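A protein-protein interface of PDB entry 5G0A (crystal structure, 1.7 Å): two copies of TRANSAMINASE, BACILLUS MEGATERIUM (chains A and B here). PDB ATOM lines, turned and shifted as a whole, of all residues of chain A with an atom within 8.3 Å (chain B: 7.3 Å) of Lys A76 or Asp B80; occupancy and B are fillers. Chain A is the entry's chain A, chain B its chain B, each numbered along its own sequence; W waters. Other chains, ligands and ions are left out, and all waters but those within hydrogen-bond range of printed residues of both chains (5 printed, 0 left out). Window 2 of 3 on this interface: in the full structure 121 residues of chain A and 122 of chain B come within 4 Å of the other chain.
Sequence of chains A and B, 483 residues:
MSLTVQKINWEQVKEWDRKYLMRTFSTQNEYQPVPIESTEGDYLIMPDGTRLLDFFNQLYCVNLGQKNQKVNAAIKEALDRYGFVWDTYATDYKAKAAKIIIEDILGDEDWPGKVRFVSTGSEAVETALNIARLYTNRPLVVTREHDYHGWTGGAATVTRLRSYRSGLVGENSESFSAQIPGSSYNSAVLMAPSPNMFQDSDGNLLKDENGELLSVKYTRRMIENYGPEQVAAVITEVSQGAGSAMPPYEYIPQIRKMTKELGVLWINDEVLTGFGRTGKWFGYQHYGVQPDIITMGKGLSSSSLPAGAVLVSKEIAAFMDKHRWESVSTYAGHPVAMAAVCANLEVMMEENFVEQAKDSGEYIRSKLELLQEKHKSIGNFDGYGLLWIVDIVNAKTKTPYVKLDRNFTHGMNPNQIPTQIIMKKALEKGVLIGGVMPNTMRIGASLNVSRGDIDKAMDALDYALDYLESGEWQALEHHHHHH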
ATOM      1  N   GLU A  37     -16.858 -12.547  -5.573  1.00  0.00           N
ATOM      2  CA  GLU A  37     -16.907 -11.276  -6.285  1.00  0.00           C
ATOM      3  C   GLU A  37     -16.095 -11.291  -7.586  1.00  0.00           C
ATOM      4  O   GLU A  37     -16.451 -10.621  -8.560  1.00  0.00           O
ATOM      5  CB  GLU A  37     -16.398 -10.170  -5.332  1.00  0.00           C
ATOM      6  CG  GLU A  37     -16.281  -8.788  -5.952  1.00  0.00           C
ATOM      7  CD  GLU A  37     -14.967  -8.571  -6.689  1.00  0.00           C
ATOM      8  OE1 GLU A  37     -13.932  -9.146  -6.284  1.00  0.00           O
ATOM      9  OE2 GLU A  37     -14.980  -7.818  -7.680  1.00  0.00           O
ATOM     10  N   SER A  38     -14.979 -12.023  -7.598  1.00  0.00           N
ATOM     11  CA  SER A  38     -14.105 -12.114  -8.778  1.00  0.00           C
ATOM     12  C   SER A  38     -13.231 -13.356  -8.707  1.00  0.00           C
ATOM     13  O   SER A  38     -13.174 -14.026  -7.670  1.00  0.00           O
ATOM     14  CB  SER A  38     -13.224 -10.848  -8.943  1.00  0.00           C
ATOM     15  OG  SER A  38     -12.294 -10.728  -7.866  1.00  0.00           O
ATOM     16  N   THR A  39     -12.543 -13.675  -9.814  1.00  0.00           N
ATOM     17  CA  THR A  39     -11.639 -14.797  -9.844  1.00  0.00           C
ATOM     18  C   THR A  39     -10.374 -14.405 -10.616  1.00  0.00           C
ATOM     19  O   THR A  39     -10.389 -13.453 -11.394  1.00  0.00           O
ATOM     20  CB  THR A  39     -12.290 -16.017 -10.534  1.00  0.00           C
ATOM     21  OG1 THR A  39     -12.514 -15.721 -11.911  1.00  0.00           O
ATOM     22  CG2 THR A  39     -13.624 -16.388  -9.839  1.00  0.00           C
ATOM     23  N   GLU A  40      -9.301 -15.157 -10.403  1.00  0.00           N
ATOM     24  CA  GLU A  40      -8.039 -14.936 -11.115  1.00  0.00           C
ATOM     25  C   GLU A  40      -7.176 -16.176 -10.935  1.00  0.00           C
ATOM     26  O   GLU A  40      -6.907 -16.590  -9.799  1.00  0.00           O
ATOM     27  CB  GLU A  40      -7.317 -13.676 -10.575  1.00  0.00           C
ATOM     28  CG  GLU A  40      -7.251 -13.575  -9.054  1.00  0.00           C
ATOM     29  CD  GLU A  40      -6.638 -12.279  -8.532  1.00  0.00           C
ATOM     30  OE1 GLU A  40      -7.171 -11.181  -8.824  1.00  0.00           O
ATOM     31  OE2 GLU A  40      -5.625 -12.367  -7.797  1.00  0.00           O
ATOM     32  N   LYS A  67     -10.243 -16.454 -15.665  1.00  0.00           N
ATOM     33  CA  LYS A  67     -10.197 -15.087 -16.186  1.00  0.00           C
ATOM     34  C   LYS A  67      -8.887 -14.853 -16.931  1.00  0.00           C
ATOM     35  O   LYS A  67      -8.137 -13.897 -16.661  1.00  0.00           O
ATOM     36  CB  LYS A  67     -10.438 -14.051 -15.059  1.00  0.00           C
ATOM     37  CG  LYS A  67     -10.841 -12.654 -15.543  1.00  0.00           C
ATOM     38  CD  LYS A  67     -11.192 -11.728 -14.381  1.00  0.00           C
ATOM     39  CE  LYS A  67      -9.959 -11.223 -13.640  1.00  0.00           C
ATOM     40  NZ  LYS A  67     -10.396 -10.688 -12.316  1.00  0.00           N
ATOM     41  N   GLN A  69      -6.629 -13.415 -19.481  1.00  0.00           N
ATOM     42  CA  GLN A  69      -6.766 -12.116 -20.149  1.00  0.00           C
ATOM     43  C   GLN A  69      -6.823 -12.174 -21.667  1.00  0.00           C
ATOM     44  O   GLN A  69      -7.465 -11.327 -22.299  1.00  0.00           O
ATOM     45  CB  GLN A  69      -5.652 -11.153 -19.703  1.00  0.00           C
ATOM     46  CG  GLN A  69      -5.672 -10.919 -18.204  1.00  0.00           C
ATOM     47  CD  GLN A  69      -6.908 -10.173 -17.764  1.00  0.00           C
ATOM     48  OE1 GLN A  69      -6.991  -8.955 -17.911  1.00  0.00           O
ATOM     49  NE2 GLN A  69      -7.885 -10.898 -17.230  1.00  0.00           N
ATOM     50  N   LYS A  70      -6.140 -13.151 -22.250  1.00  0.00           N
ATOM     51  CA  LYS A  70      -6.149 -13.306 -23.701  1.00  0.00           C
ATOM     52  C   LYS A  70      -7.508 -13.800 -24.176  1.00  0.00           C
ATOM     53  O   LYS A  70      -8.022 -13.349 -25.198  1.00  0.00           O
ATOM     54  CB  LYS A  70      -5.039 -14.264 -24.164  1.00  0.00           C
ATOM     55  CG  LYS A  70      -3.641 -13.760 -23.827  1.00  0.00           C
ATOM     56  CD  LYS A  70      -2.557 -14.634 -24.451  1.00  0.00           C
ATOM     57  CE  LYS A  70      -1.183 -14.219 -23.937  1.00  0.00           C
ATOM     58  NZ  LYS A  70      -0.091 -14.668 -24.847  1.00  0.00           N
ATOM     59  N   VAL A  71      -8.095 -14.721 -23.418  1.00  0.00           N
ATOM     60  CA  VAL A  71      -9.439 -15.192 -23.736  1.00  0.00           C
ATOM     61  C   VAL A  71     -10.434 -14.041 -23.576  1.00  0.00           C
ATOM     62  O   VAL A  71     -11.266 -13.807 -24.456  1.00  0.00           O
ATOM     63  CB  VAL A  71      -9.859 -16.422 -22.886  1.00  0.00           C
ATOM     64  CG1 VAL A  71     -11.325 -16.803 -23.177  1.00  0.00           C
ATOM     65  CG2 VAL A  71      -8.955 -17.601 -23.194  1.00  0.00           C
ATOM     66  N   ASN A  72     -10.359 -13.333 -22.454  1.00  0.00           N
ATOM     67  CA  ASN A  72     -11.295 -12.245 -22.242  1.00  0.00           C
ATOM     68  C   ASN A  72     -11.161 -11.162 -23.313  1.00  0.00           C
ATOM     69  O   ASN A  72     -12.159 -10.661 -23.789  1.00  0.00           O
ATOM     70  CB  ASN A  72     -11.263 -11.734 -20.798  1.00  0.00           C
ATOM     71  CG  ASN A  72     -11.946 -12.697 -19.842  1.00  0.00           C
ATOM     72  OD1 ASN A  72     -12.212 -13.850 -20.196  1.00  0.00           O
ATOM     73  ND2 ASN A  72     -12.223 -12.242 -18.621  1.00  0.00           N
ATOM     74  N   ALA A  73      -9.933 -10.899 -23.767  1.00  0.00           N
ATOM     75  CA  ALA A  73      -9.696  -9.936 -24.855  1.00  0.00           C
ATOM     76  C   ALA A  73     -10.327 -10.412 -26.152  1.00  0.00           C
ATOM     77  O   ALA A  73     -10.929  -9.622 -26.898  1.00  0.00           O
ATOM     78  CB  ALA A  73      -8.192  -9.688 -25.038  1.00  0.00           C
ATOM     79  N   ALA A  74     -10.226 -11.718 -26.409  1.00  0.00           N
ATOM     80  CA  ALA A  74     -10.811 -12.328 -27.597  1.00  0.00           C
ATOM     81  C   ALA A  74     -12.352 -12.251 -27.601  1.00  0.00           C
ATOM     82  O   ALA A  74     -12.975 -12.009 -28.656  1.00  0.00           O
ATOM     83  CB  ALA A  74     -10.345 -13.763 -27.734  1.00  0.00           C
ATOM     84  N   ILE A  75     -12.957 -12.465 -26.437  1.00  0.00           N
ATOM     85  CA  ILE A  75     -14.414 -12.285 -26.283  1.00  0.00           C
ATOM     86  C   ILE A  75     -14.818 -10.854 -26.555  1.00  0.00           C
ATOM     87  O   ILE A  75     -15.748 -10.614 -27.313  1.00  0.00           O
ATOM     88  CB  ILE A  75     -14.934 -12.711 -24.883  1.00  0.00           C
ATOM     89  CG1 ILE A  75     -14.678 -14.209 -24.682  1.00  0.00           C
ATOM     90  CG2 ILE A  75     -16.422 -12.360 -24.741  1.00  0.00           C
ATOM     91  CD1 ILE A  75     -14.798 -14.682 -23.235  1.00  0.00           C
ATOM     92  N   LYS A  76     -14.095  -9.906 -25.964  1.00  0.00           N
ATOM     93  CA  LYS A  76     -14.360  -8.480 -26.212  1.00  0.00           C
ATOM     94  C   LYS A  76     -14.282  -8.129 -27.692  1.00  0.00           C
ATOM     95  O   LYS A  76     -15.134  -7.392 -28.196  1.00  0.00           O
ATOM     96  CB  LYS A  76     -13.433  -7.599 -25.368  1.00  0.00           C
ATOM     97  CG  LYS A  76     -13.693  -7.699 -23.866  1.00  0.00           C
ATOM     98  CD  LYS A  76     -12.806  -6.725 -23.082  1.00  0.00           C
ATOM     99  CE  LYS A  76     -12.963  -6.890 -21.577  1.00  0.00           C
ATOM    100  NZ  LYS A  76     -12.155  -5.861 -20.835  1.00  0.00           N
ATOM    101  N   GLU A  77     -13.294  -8.678 -28.400  1.00  0.00           N
ATOM    102  CA  GLU A  77     -13.193  -8.480 -29.849  1.00  0.00           C
ATOM    103  C   GLU A  77     -14.386  -9.025 -30.609  1.00  0.00           C
ATOM    104  O   GLU A  77     -14.895  -8.377 -31.511  1.00  0.00           O
ATOM    105  CB  GLU A  77     -11.926  -9.112 -30.428  1.00  0.00           C
ATOM    106  CG  GLU A  77     -10.688  -8.267 -30.277  1.00  0.00           C
ATOM    107  CD  GLU A  77      -9.496  -8.834 -31.040  1.00  0.00           C
ATOM    108  OE1 GLU A  77      -9.690  -9.633 -31.993  1.00  0.00           O
ATOM    109  OE2 GLU A  77      -8.355  -8.476 -30.683  1.00  0.00           O
ATOM    110  N   ALA A  78     -14.842 -10.226 -30.240  1.00  0.00           N
ATOM    111  CA  ALA A  78     -16.010 -10.810 -30.872  1.00  0.00           C
ATOM    112  C   ALA A  78     -17.244  -9.926 -30.668  1.00  0.00           C
ATOM    113  O   ALA A  78     -18.079  -9.832 -31.546  1.00  0.00           O
ATOM    114  CB  ALA A  78     -16.268 -12.217 -30.327  1.00  0.00           C
ATOM    115  N   LEU A  79     -17.332  -9.286 -29.508  1.00  0.00           N
ATOM    116  CA  LEU A  79     -18.469  -8.425 -29.155  1.00  0.00           C
ATOM    117  C   LEU A  79     -18.452  -7.080 -29.888  1.00  0.00           C
ATOM    118  O   LEU A  79     -19.373  -6.274 -29.760  1.00  0.00           O
ATOM    119  CB  LEU A  79     -18.494  -8.212 -27.636  1.00  0.00           C
ATOM    120  CG  LEU A  79     -18.872  -9.439 -26.785  1.00  0.00           C
ATOM    121  CD1 LEU A  79     -18.554  -9.202 -25.319  1.00  0.00           C
ATOM    122  CD2 LEU A  79     -20.342  -9.832 -26.973  1.00  0.00           C
ATOM    123  N   ASP A  80     -17.399  -6.838 -30.665  1.00  0.00           N
ATOM    124  CA  ASP A  80     -17.391  -5.670 -31.537  1.00  0.00           C
ATOM    125  C   ASP A  80     -18.026  -6.013 -32.873  1.00  0.00           C
ATOM    126  O   ASP A  80     -18.292  -5.122 -33.669  1.00  0.00           O
ATOM    127  CB  ASP A  80     -15.965  -5.168 -31.770  1.00  0.00           C
ATOM    128  CG  ASP A  80     -15.370  -4.522 -30.540  1.00  0.00           C
ATOM    129  OD1 ASP A  80     -16.140  -4.052 -29.678  1.00  0.00           O
ATOM    130  OD2 ASP A  80     -14.120  -4.497 -30.452  1.00  0.00           O
ATOM    131  N   ARG A  81     -18.252  -7.307 -33.111  1.00  0.00           N
ATOM    132  CA  ARG A  81     -18.818  -7.782 -34.372  1.00  0.00           C
ATOM    133  C   ARG A  81     -20.204  -8.401 -34.170  1.00  0.00           C
ATOM    134  O   ARG A  81     -21.077  -8.273 -35.012  1.00  0.00           O
ATOM    135  CB  ARG A  81     -17.885  -8.788 -35.022  1.00  0.00           C
ATOM    136  CG  ARG A  81     -16.608  -8.169 -35.612  1.00  0.00           C
ATOM    137  CD  ARG A  81     -15.636  -9.244 -36.067  1.00  0.00           C
ATOM    138  NE  ARG A  81     -16.242 -10.234 -36.965  1.00  0.00           N
ATOM    139  CZ  ARG A  81     -15.774 -11.466 -37.163  1.00  0.00           C
ATOM    140  NH1 ARG A  81     -14.649 -11.887 -36.566  1.00  0.00           N
ATOM    141  NH2 ARG A  81     -16.409 -12.287 -37.993  1.00  0.00           N
ATOM    142  N   TYR A  82     -20.392  -9.081 -33.050  1.00  0.00           N
ATOM    143  CA  TYR A  82     -21.630  -9.838 -32.803  1.00  0.00           C
ATOM    144  C   TYR A  82     -22.212  -9.427 -31.447  1.00  0.00           C
ATOM    145  O   TYR A  82     -21.494  -8.885 -30.615  1.00  0.00           O
ATOM    146  CB  TYR A  82     -21.343 -11.360 -32.828  1.00  0.00           C
ATOM    147  CG  TYR A  82     -20.785 -11.921 -34.131  1.00  0.00           C
ATOM    148  CD1 TYR A  82     -21.607 -12.131 -35.251  1.00  0.00           C
ATOM    149  CD2 TYR A  82     -19.440 -12.244 -34.237  1.00  0.00           C
ATOM    150  CE1 TYR A  82     -21.079 -12.652 -36.439  1.00  0.00           C
ATOM    151  CE2 TYR A  82     -18.905 -12.779 -35.396  1.00  0.00           C
ATOM    152  CZ  TYR A  82     -19.722 -12.965 -36.496  1.00  0.00           C
ATOM    153  OH  TYR A  82     -19.175 -13.482 -37.630  1.00  0.00           O
ATOM    154  N   TYR A  93     -15.337 -17.710 -36.472  1.00  0.00           N
ATOM    155  CA  TYR A  93     -15.063 -18.335 -35.165  1.00  0.00           C
ATOM    156  C   TYR A  93     -15.508 -19.811 -35.096  1.00  0.00           C
ATOM    157  O   TYR A  93     -14.775 -20.645 -34.567  1.00  0.00           O
ATOM    158  CB  TYR A  93     -15.748 -17.563 -34.047  1.00  0.00           C
ATOM    159  CG  TYR A  93     -15.263 -16.152 -33.884  1.00  0.00           C
ATOM    160  CD1 TYR A  93     -13.902 -15.870 -33.677  1.00  0.00           C
ATOM    161  CD2 TYR A  93     -16.172 -15.096 -33.879  1.00  0.00           C
ATOM    162  CE1 TYR A  93     -13.469 -14.564 -33.527  1.00  0.00           C
ATOM    163  CE2 TYR A  93     -15.744 -13.802 -33.686  1.00  0.00           C
ATOM    164  CZ  TYR A  93     -14.398 -13.545 -33.517  1.00  0.00           C
ATOM    165  OH  TYR A  93     -14.007 -12.245 -33.333  1.00  0.00           O
ATOM    166  N   LEU A 305     -17.043 -19.163 -21.560  1.00  0.00           N
ATOM    167  CA  LEU A 305     -18.461 -19.032 -21.920  1.00  0.00           C
ATOM    168  C   LEU A 305     -19.022 -20.431 -22.136  1.00  0.00           C
ATOM    169  O   LEU A 305     -18.251 -21.393 -22.300  1.00  0.00           O
ATOM    170  CB  LEU A 305     -18.625 -18.215 -23.213  1.00  0.00           C
ATOM    171  CG  LEU A 305     -18.299 -16.718 -23.108  1.00  0.00           C
ATOM    172  CD1 LEU A 305     -18.347 -16.125 -24.521  1.00  0.00           C
ATOM    173  CD2 LEU A 305     -19.245 -15.957 -22.173  1.00  0.00           C
ATOM    174  N   VAL A 336     -19.947 -15.818 -30.306  1.00  0.00           N
ATOM    175  CA  VAL A 336     -19.128 -15.276 -29.193  1.00  0.00           C
ATOM    176  C   VAL A 336     -18.579 -16.425 -28.352  1.00  0.00           C
ATOM    177  O   VAL A 336     -17.386 -16.421 -27.985  1.00  0.00           O
ATOM    178  CB  VAL A 336     -19.879 -14.203 -28.376  1.00  0.00           C
ATOM    179  CG1 VAL A 336     -18.979 -13.578 -27.302  1.00  0.00           C
ATOM    180  CG2 VAL A 336     -20.395 -13.095 -29.310  1.00  0.00           C
ATOM    181  N   ALA A 339     -15.776 -17.783 -30.371  1.00  0.00           N
ATOM    182  CA  ALA A 339     -14.542 -16.968 -30.243  1.00  0.00           C
ATOM    183  C   ALA A 339     -13.774 -17.317 -28.966  1.00  0.00           C
ATOM    184  O   ALA A 339     -12.542 -17.364 -28.962  1.00  0.00           O
ATOM    185  CB  ALA A 339     -14.862 -15.488 -30.304  1.00  0.00           C
ATOM    186  N   ALA A 340     -14.514 -17.601 -27.897  1.00  0.00           N
ATOM    187  CA  ALA A 340     -13.920 -18.019 -26.632  1.00  0.00           C
ATOM    188  C   ALA A 340     -13.216 -19.372 -26.771  1.00  0.00           C
ATOM    189  O   ALA A 340     -12.091 -19.542 -26.279  1.00  0.00           O
ATOM    190  CB  ALA A 340     -14.980 -18.039 -25.523  1.00  0.00           C
ATOM    191  N   ASN B  72     -23.482  -5.256 -24.691  1.00  0.00           N
ATOM    192  CA  ASN B  72     -22.112  -5.680 -24.929  1.00  0.00           C
ATOM    193  C   ASN B  72     -21.105  -5.001 -23.995  1.00  0.00           C
ATOM    194  O   ASN B  72     -20.167  -5.651 -23.517  1.00  0.00           O
ATOM    195  CB  ASN B  72     -21.769  -5.558 -26.418  1.00  0.00           C
ATOM    196  CG  ASN B  72     -22.405  -6.667 -27.248  1.00  0.00           C
ATOM    197  OD1 ASN B  72     -23.313  -7.372 -26.777  1.00  0.00           O
ATOM    198  ND2 ASN B  72     -21.911  -6.857 -28.468  1.00  0.00           N
ATOM    199  N   ALA B  74     -21.855  -4.100 -20.973  1.00  0.00           N
ATOM    200  CA  ALA B  74     -22.089  -4.773 -19.706  1.00  0.00           C
ATOM    201  C   ALA B  74     -21.345  -6.119 -19.648  1.00  0.00           C
ATOM    202  O   ALA B  74     -20.803  -6.473 -18.626  1.00  0.00           O
ATOM    203  CB  ALA B  74     -23.577  -4.973 -19.467  1.00  0.00           C
ATOM    204  N   ILE B  75     -21.350  -6.871 -20.743  1.00  0.00           N
ATOM    205  CA  ILE B  75     -20.595  -8.117 -20.776  1.00  0.00           C
ATOM    206  C   ILE B  75     -19.105  -7.854 -20.636  1.00  0.00           C
ATOM    207  O   ILE B  75     -18.421  -8.562 -19.911  1.00  0.00           O
ATOM    208  CB  ILE B  75     -20.881  -8.932 -22.046  1.00  0.00           C
ATOM    209  CG1 ILE B  75     -22.366  -9.342 -22.085  1.00  0.00           C
ATOM    210  CG2 ILE B  75     -20.038 -10.205 -22.085  1.00  0.00           C
ATOM    211  CD1 ILE B  75     -22.828  -9.786 -23.462  1.00  0.00           C
ATOM    212  N   LYS B  76     -18.607  -6.824 -21.329  1.00  0.00           N
ATOM    213  CA  LYS B  76     -17.174  -6.509 -21.229  1.00  0.00           C
ATOM    214  C   LYS B  76     -16.818  -6.146 -19.778  1.00  0.00           C
ATOM    215  O   LYS B  76     -15.759  -6.529 -19.288  1.00  0.00           O
ATOM    216  CB  LYS B  76     -16.790  -5.373 -22.185  1.00  0.00           C
ATOM    217  CG  LYS B  76     -16.816  -5.762 -23.653  1.00  0.00           C
ATOM    218  CD  LYS B  76     -16.447  -4.554 -24.528  1.00  0.00           C
ATOM    219  CE  LYS B  76     -16.555  -4.913 -26.004  1.00  0.00           C
ATOM    220  NZ  LYS B  76     -16.238  -3.762 -26.909  1.00  0.00           N
ATOM    221  N   GLU B  77     -17.709  -5.421 -19.101  1.00  0.00           N
ATOM    222  CA  GLU B  77     -17.530  -5.090 -17.686  1.00  0.00           C
ATOM    223  C   GLU B  77     -17.449  -6.323 -16.780  1.00  0.00           C
ATOM    224  O   GLU B  77     -16.603  -6.393 -15.908  1.00  0.00           O
ATOM    225  CB  GLU B  77     -18.630  -4.156 -17.176  1.00  0.00           C
ATOM    226  CG  GLU B  77     -18.329  -2.670 -17.257  1.00  0.00           C
ATOM    227  CD  GLU B  77     -18.914  -1.894 -16.077  1.00  0.00           C
ATOM    228  OE1 GLU B  77     -19.820  -2.414 -15.388  1.00  0.00           O
ATOM    229  OE2 GLU B  77     -18.459  -0.758 -15.818  1.00  0.00           O
ATOM    230  N   ALA B  78     -18.346  -7.290 -16.970  1.00  0.00           N
ATOM    231  CA  ALA B  78     -18.327  -8.509 -16.150  1.00  0.00           C
ATOM    232  C   ALA B  78     -17.003  -9.277 -16.301  1.00  0.00           C
ATOM    233  O   ALA B  78     -16.549  -9.953 -15.381  1.00  0.00           O
ATOM    234  CB  ALA B  78     -19.488  -9.424 -16.532  1.00  0.00           C
ATOM    235  N   LEU B  79     -16.433  -9.210 -17.496  1.00  0.00           N
ATOM    236  CA  LEU B  79     -15.150  -9.854 -17.782  1.00  0.00           C
ATOM    237  C   LEU B  79     -13.941  -9.211 -17.061  1.00  0.00           C
ATOM    238  O   LEU B  79     -12.851  -9.787 -17.063  1.00  0.00           O
ATOM    239  CB  LEU B  79     -14.914  -9.895 -19.290  1.00  0.00           C
ATOM    240  CG  LEU B  79     -15.823 -10.815 -20.135  1.00  0.00           C
ATOM    241  CD1 LEU B  79     -15.702 -10.420 -21.605  1.00  0.00           C
ATOM    242  CD2 LEU B  79     -15.574 -12.304 -19.931  1.00  0.00           C
ATOM    243  N   ASP B  80     -14.129  -8.037 -16.446  1.00  0.00           N
ATOM    244  CA  ASP B  80     -13.110  -7.497 -15.526  1.00  0.00           C
ATOM    245  C   ASP B  80     -13.035  -8.320 -14.252  1.00  0.00           C
ATOM    246  O   ASP B  80     -12.011  -8.311 -13.544  1.00  0.00           O
ATOM    247  CB  ASP B  80     -13.444  -6.052 -15.121  1.00  0.00           C
ATOM    248  CG  ASP B  80     -13.225  -5.049 -16.241  1.00  0.00           C
ATOM    249  OD1 ASP B  80     -12.517  -5.364 -17.223  1.00  0.00           O
ATOM    250  OD2 ASP B  80     -13.768  -3.929 -16.116  1.00  0.00           O
ATOM    251  N   ARG B  81     -14.124  -9.035 -13.944  1.00  0.00           N
ATOM    252  CA  ARG B  81     -14.213  -9.759 -12.675  1.00  0.00           C
ATOM    253  C   ARG B  81     -14.191 -11.284 -12.822  1.00  0.00           C
ATOM    254  O   ARG B  81     -13.627 -11.991 -11.979  1.00  0.00           O
ATOM    255  CB  ARG B  81     -15.480  -9.339 -11.915  1.00  0.00           C
ATOM    256  CG  ARG B  81     -15.396  -7.934 -11.306  1.00  0.00           C
ATOM    257  CD  ARG B  81     -16.786  -7.428 -10.942  1.00  0.00           C
ATOM    258  NE  ARG B  81     -17.404  -8.338  -9.991  1.00  0.00           N
ATOM    259  CZ  ARG B  81     -18.712  -8.483  -9.798  1.00  0.00           C
ATOM    260  NH1 ARG B  81     -19.600  -7.758 -10.477  1.00  0.00           N
ATOM    261  NH2 ARG B  81     -19.121  -9.369  -8.911  1.00  0.00           N
ATOM    262  N   TYR B  82     -14.826 -11.774 -13.891  1.00  0.00           N
ATOM    263  CA  TYR B  82     -14.987 -13.199 -14.120  1.00  0.00           C
ATOM    264  C   TYR B  82     -14.413 -13.596 -15.493  1.00  0.00           C
ATOM    265  O   TYR B  82     -14.373 -12.758 -16.390  1.00  0.00           O
ATOM    266  CB  TYR B  82     -16.492 -13.512 -14.080  1.00  0.00           C
ATOM    267  CG  TYR B  82     -17.163 -13.194 -12.756  1.00  0.00           C
ATOM    268  CD1 TYR B  82     -16.913 -13.981 -11.616  1.00  0.00           C
ATOM    269  CD2 TYR B  82     -18.078 -12.141 -12.653  1.00  0.00           C
ATOM    270  CE1 TYR B  82     -17.542 -13.713 -10.404  1.00  0.00           C
ATOM    271  CE2 TYR B  82     -18.717 -11.864 -11.452  1.00  0.00           C
ATOM    272  CZ  TYR B  82     -18.443 -12.644 -10.329  1.00  0.00           C
ATOM    273  OH  TYR B  82     -19.084 -12.373  -9.139  1.00  0.00           O
ATOM    274  N   GLY B  83     -13.990 -14.853 -15.695  1.00  0.00           N
ATOM    275  CA  GLY B  83     -14.035 -15.923 -14.701  1.00  0.00           C
ATOM    276  C   GLY B  83     -15.281 -16.794 -14.785  1.00  0.00           C
ATOM    277  O   GLY B  83     -16.191 -16.565 -15.598  1.00  0.00           O
ATOM    278  N   TYR B  93     -24.630 -10.878 -10.236  1.00  0.00           N
ATOM    279  CA  TYR B  93     -25.338 -10.937 -11.514  1.00  0.00           C
ATOM    280  C   TYR B  93     -26.460 -11.981 -11.497  1.00  0.00           C
ATOM    281  O   TYR B  93     -27.572 -11.731 -11.997  1.00  0.00           O
ATOM    282  CB  TYR B  93     -24.378 -11.264 -12.652  1.00  0.00           C
ATOM    283  CG  TYR B  93     -23.351 -10.195 -12.951  1.00  0.00           C
ATOM    284  CD1 TYR B  93     -23.733  -8.878 -13.220  1.00  0.00           C
ATOM    285  CD2 TYR B  93     -22.003 -10.519 -12.997  1.00  0.00           C
ATOM    286  CE1 TYR B  93     -22.778  -7.897 -13.505  1.00  0.00           C
ATOM    287  CE2 TYR B  93     -21.038  -9.552 -13.283  1.00  0.00           C
ATOM    288  CZ  TYR B  93     -21.433  -8.247 -13.541  1.00  0.00           C
ATOM    289  OH  TYR B  93     -20.456  -7.292 -13.852  1.00  0.00           O
ATOM    290  N   VAL B 336     -21.073 -14.542 -16.327  1.00  0.00           N
ATOM    291  CA  VAL B 336     -21.004 -13.601 -17.467  1.00  0.00           C
ATOM    292  C   VAL B 336     -22.296 -13.668 -18.290  1.00  0.00           C
ATOM    293  O   VAL B 336     -22.819 -12.636 -18.731  1.00  0.00           O
ATOM    294  CB  VAL B 336     -19.774 -13.866 -18.351  1.00  0.00           C
ATOM    295  CG1 VAL B 336     -19.716 -12.894 -19.528  1.00  0.00           C
ATOM    296  CG2 VAL B 336     -18.499 -13.758 -17.516  1.00  0.00           C
HETATM  297  O   HOH W   1     -11.210  -8.406 -10.686  1.00  0.00           O
HETATM  298  O   HOH W   2     -10.987  -8.543 -19.419  1.00  0.00           O
HETATM  299  O   HOH W   3     -12.477 -17.744 -16.753  1.00  0.00           O
HETATM  300  O   HOH W   4     -13.125 -15.507 -18.580  1.00  0.00           O
HETATM  301  O   HOH W   5     -10.199  -9.201 -16.820  1.00  0.00           O
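O of Tyr A82 is in hydrogen-bond range of ND2 of Asn B72, at 3.0 Å.
The side-chain amide nitrogen (ND2) of Asn A72 is in hydrogen-bond range of the backbone carbonyl oxygen (O) of Leu B79, 3.0 Å away.
The side-chain amino group (NZ) of Lys A76 lies within salt-bridge range of the side-chain carboxylate (OD1) of Asp B80 (3.7 Å).
N of Thr A39 sits at hydrogen-bond distance from O of Arg B81 (2.9 Å).
The backbone carbonyl oxygen of Glu A37 sits at hydrogen-bond distance from the side-chain hydroxyl of Tyr B82, at 3.2 Å.
NZ of Lys A67 lies within hydrogen-bond range of O of Asp B80, at 3.1 Å.
OE2 of Glu A37 lies within salt-bridge range of NE of Arg B81 (3.4 Å).
The side-chain amide nitrogen of Asn A72 sits at hydrogen-bond distance from the backbone carbonyl oxygen of Tyr B82, 3.1 Å away.
The side-chain amide nitrogen (ND2) of Asn B72 lies within hydrogen-bond range of the backbone carbonyl oxygen (O) of Leu A79, 2.9 Å away.
OD1 of Asp A80 lies within salt-bridge range of NZ of Lys B76, at 2.8 Å.
The guanidinium group (NH2) of Arg B81 sits at hydrogen-bond distance from the side-chain hydroxyl (OH) of Tyr B82 (3.0 Å).
Among the printed residues, merely in contact across the chains: Ser A38 with Arg B81, Thr A39 with Gly B83, Lys A67 with Leu B79, Lys A67 with Arg B81, Lys A67 with Tyr B82, Lys A67 with Gly B83, Ile A75 with Leu B79, Lys A76 with Lys B76 and Leu A79 with Ile B75.
Of the printed residues of chain B, Tyr A82 touches Asn B72.
Printed residues of chain A within 4 Å of Lys B76: Lys A76 and Asp A80.
Leu A305 touches none of the printed residues of chain B.
The nearest residue of chain A that does not touch Asp B80 is Asn A72 (5.1 Å).
Hydrophobic or aromatic side chains of chain B within 4 Å of the printed part of chain A: Ile B75, Leu B79 and Tyr B82.
Of the 24 printed residues of chain A, 10 touch a printed residue of chain B.
Hydrophobic or aromatic side chains of chain A that line the printed part of chain B: Ile A75 and Leu A79.
Among the printed residues, Asp or Glu carboxylates within 4 Å of a Lys or Arg side-chain nitrogen of the other chain: Glu A37 with Arg B81 (3.4 Å), Lys A76 with Asp B80 (3.7 Å) and Asp A80 with Lys B76 (2.8 Å).
Asn A72 touches Leu B79, and with the chains exchanged Leu A79 touches Asn B72.
Asn A72 touches Tyr B82, and with the chains exchanged Tyr A82 touches Asn B72.
Lys A76 touches its own counterpart, Lys B76.
Water W1 bridges the side-chain amino group (NZ) of Lys A67 (2.9 Å) and the backbone carbonyl oxygen (O) of Asp B80 (3.0 Å).
Water W2 bridges the side-chain amino group of Lys A76 (3.2 Å) and the backbone carbonyl oxygen of Leu B79 (3.3 Å).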
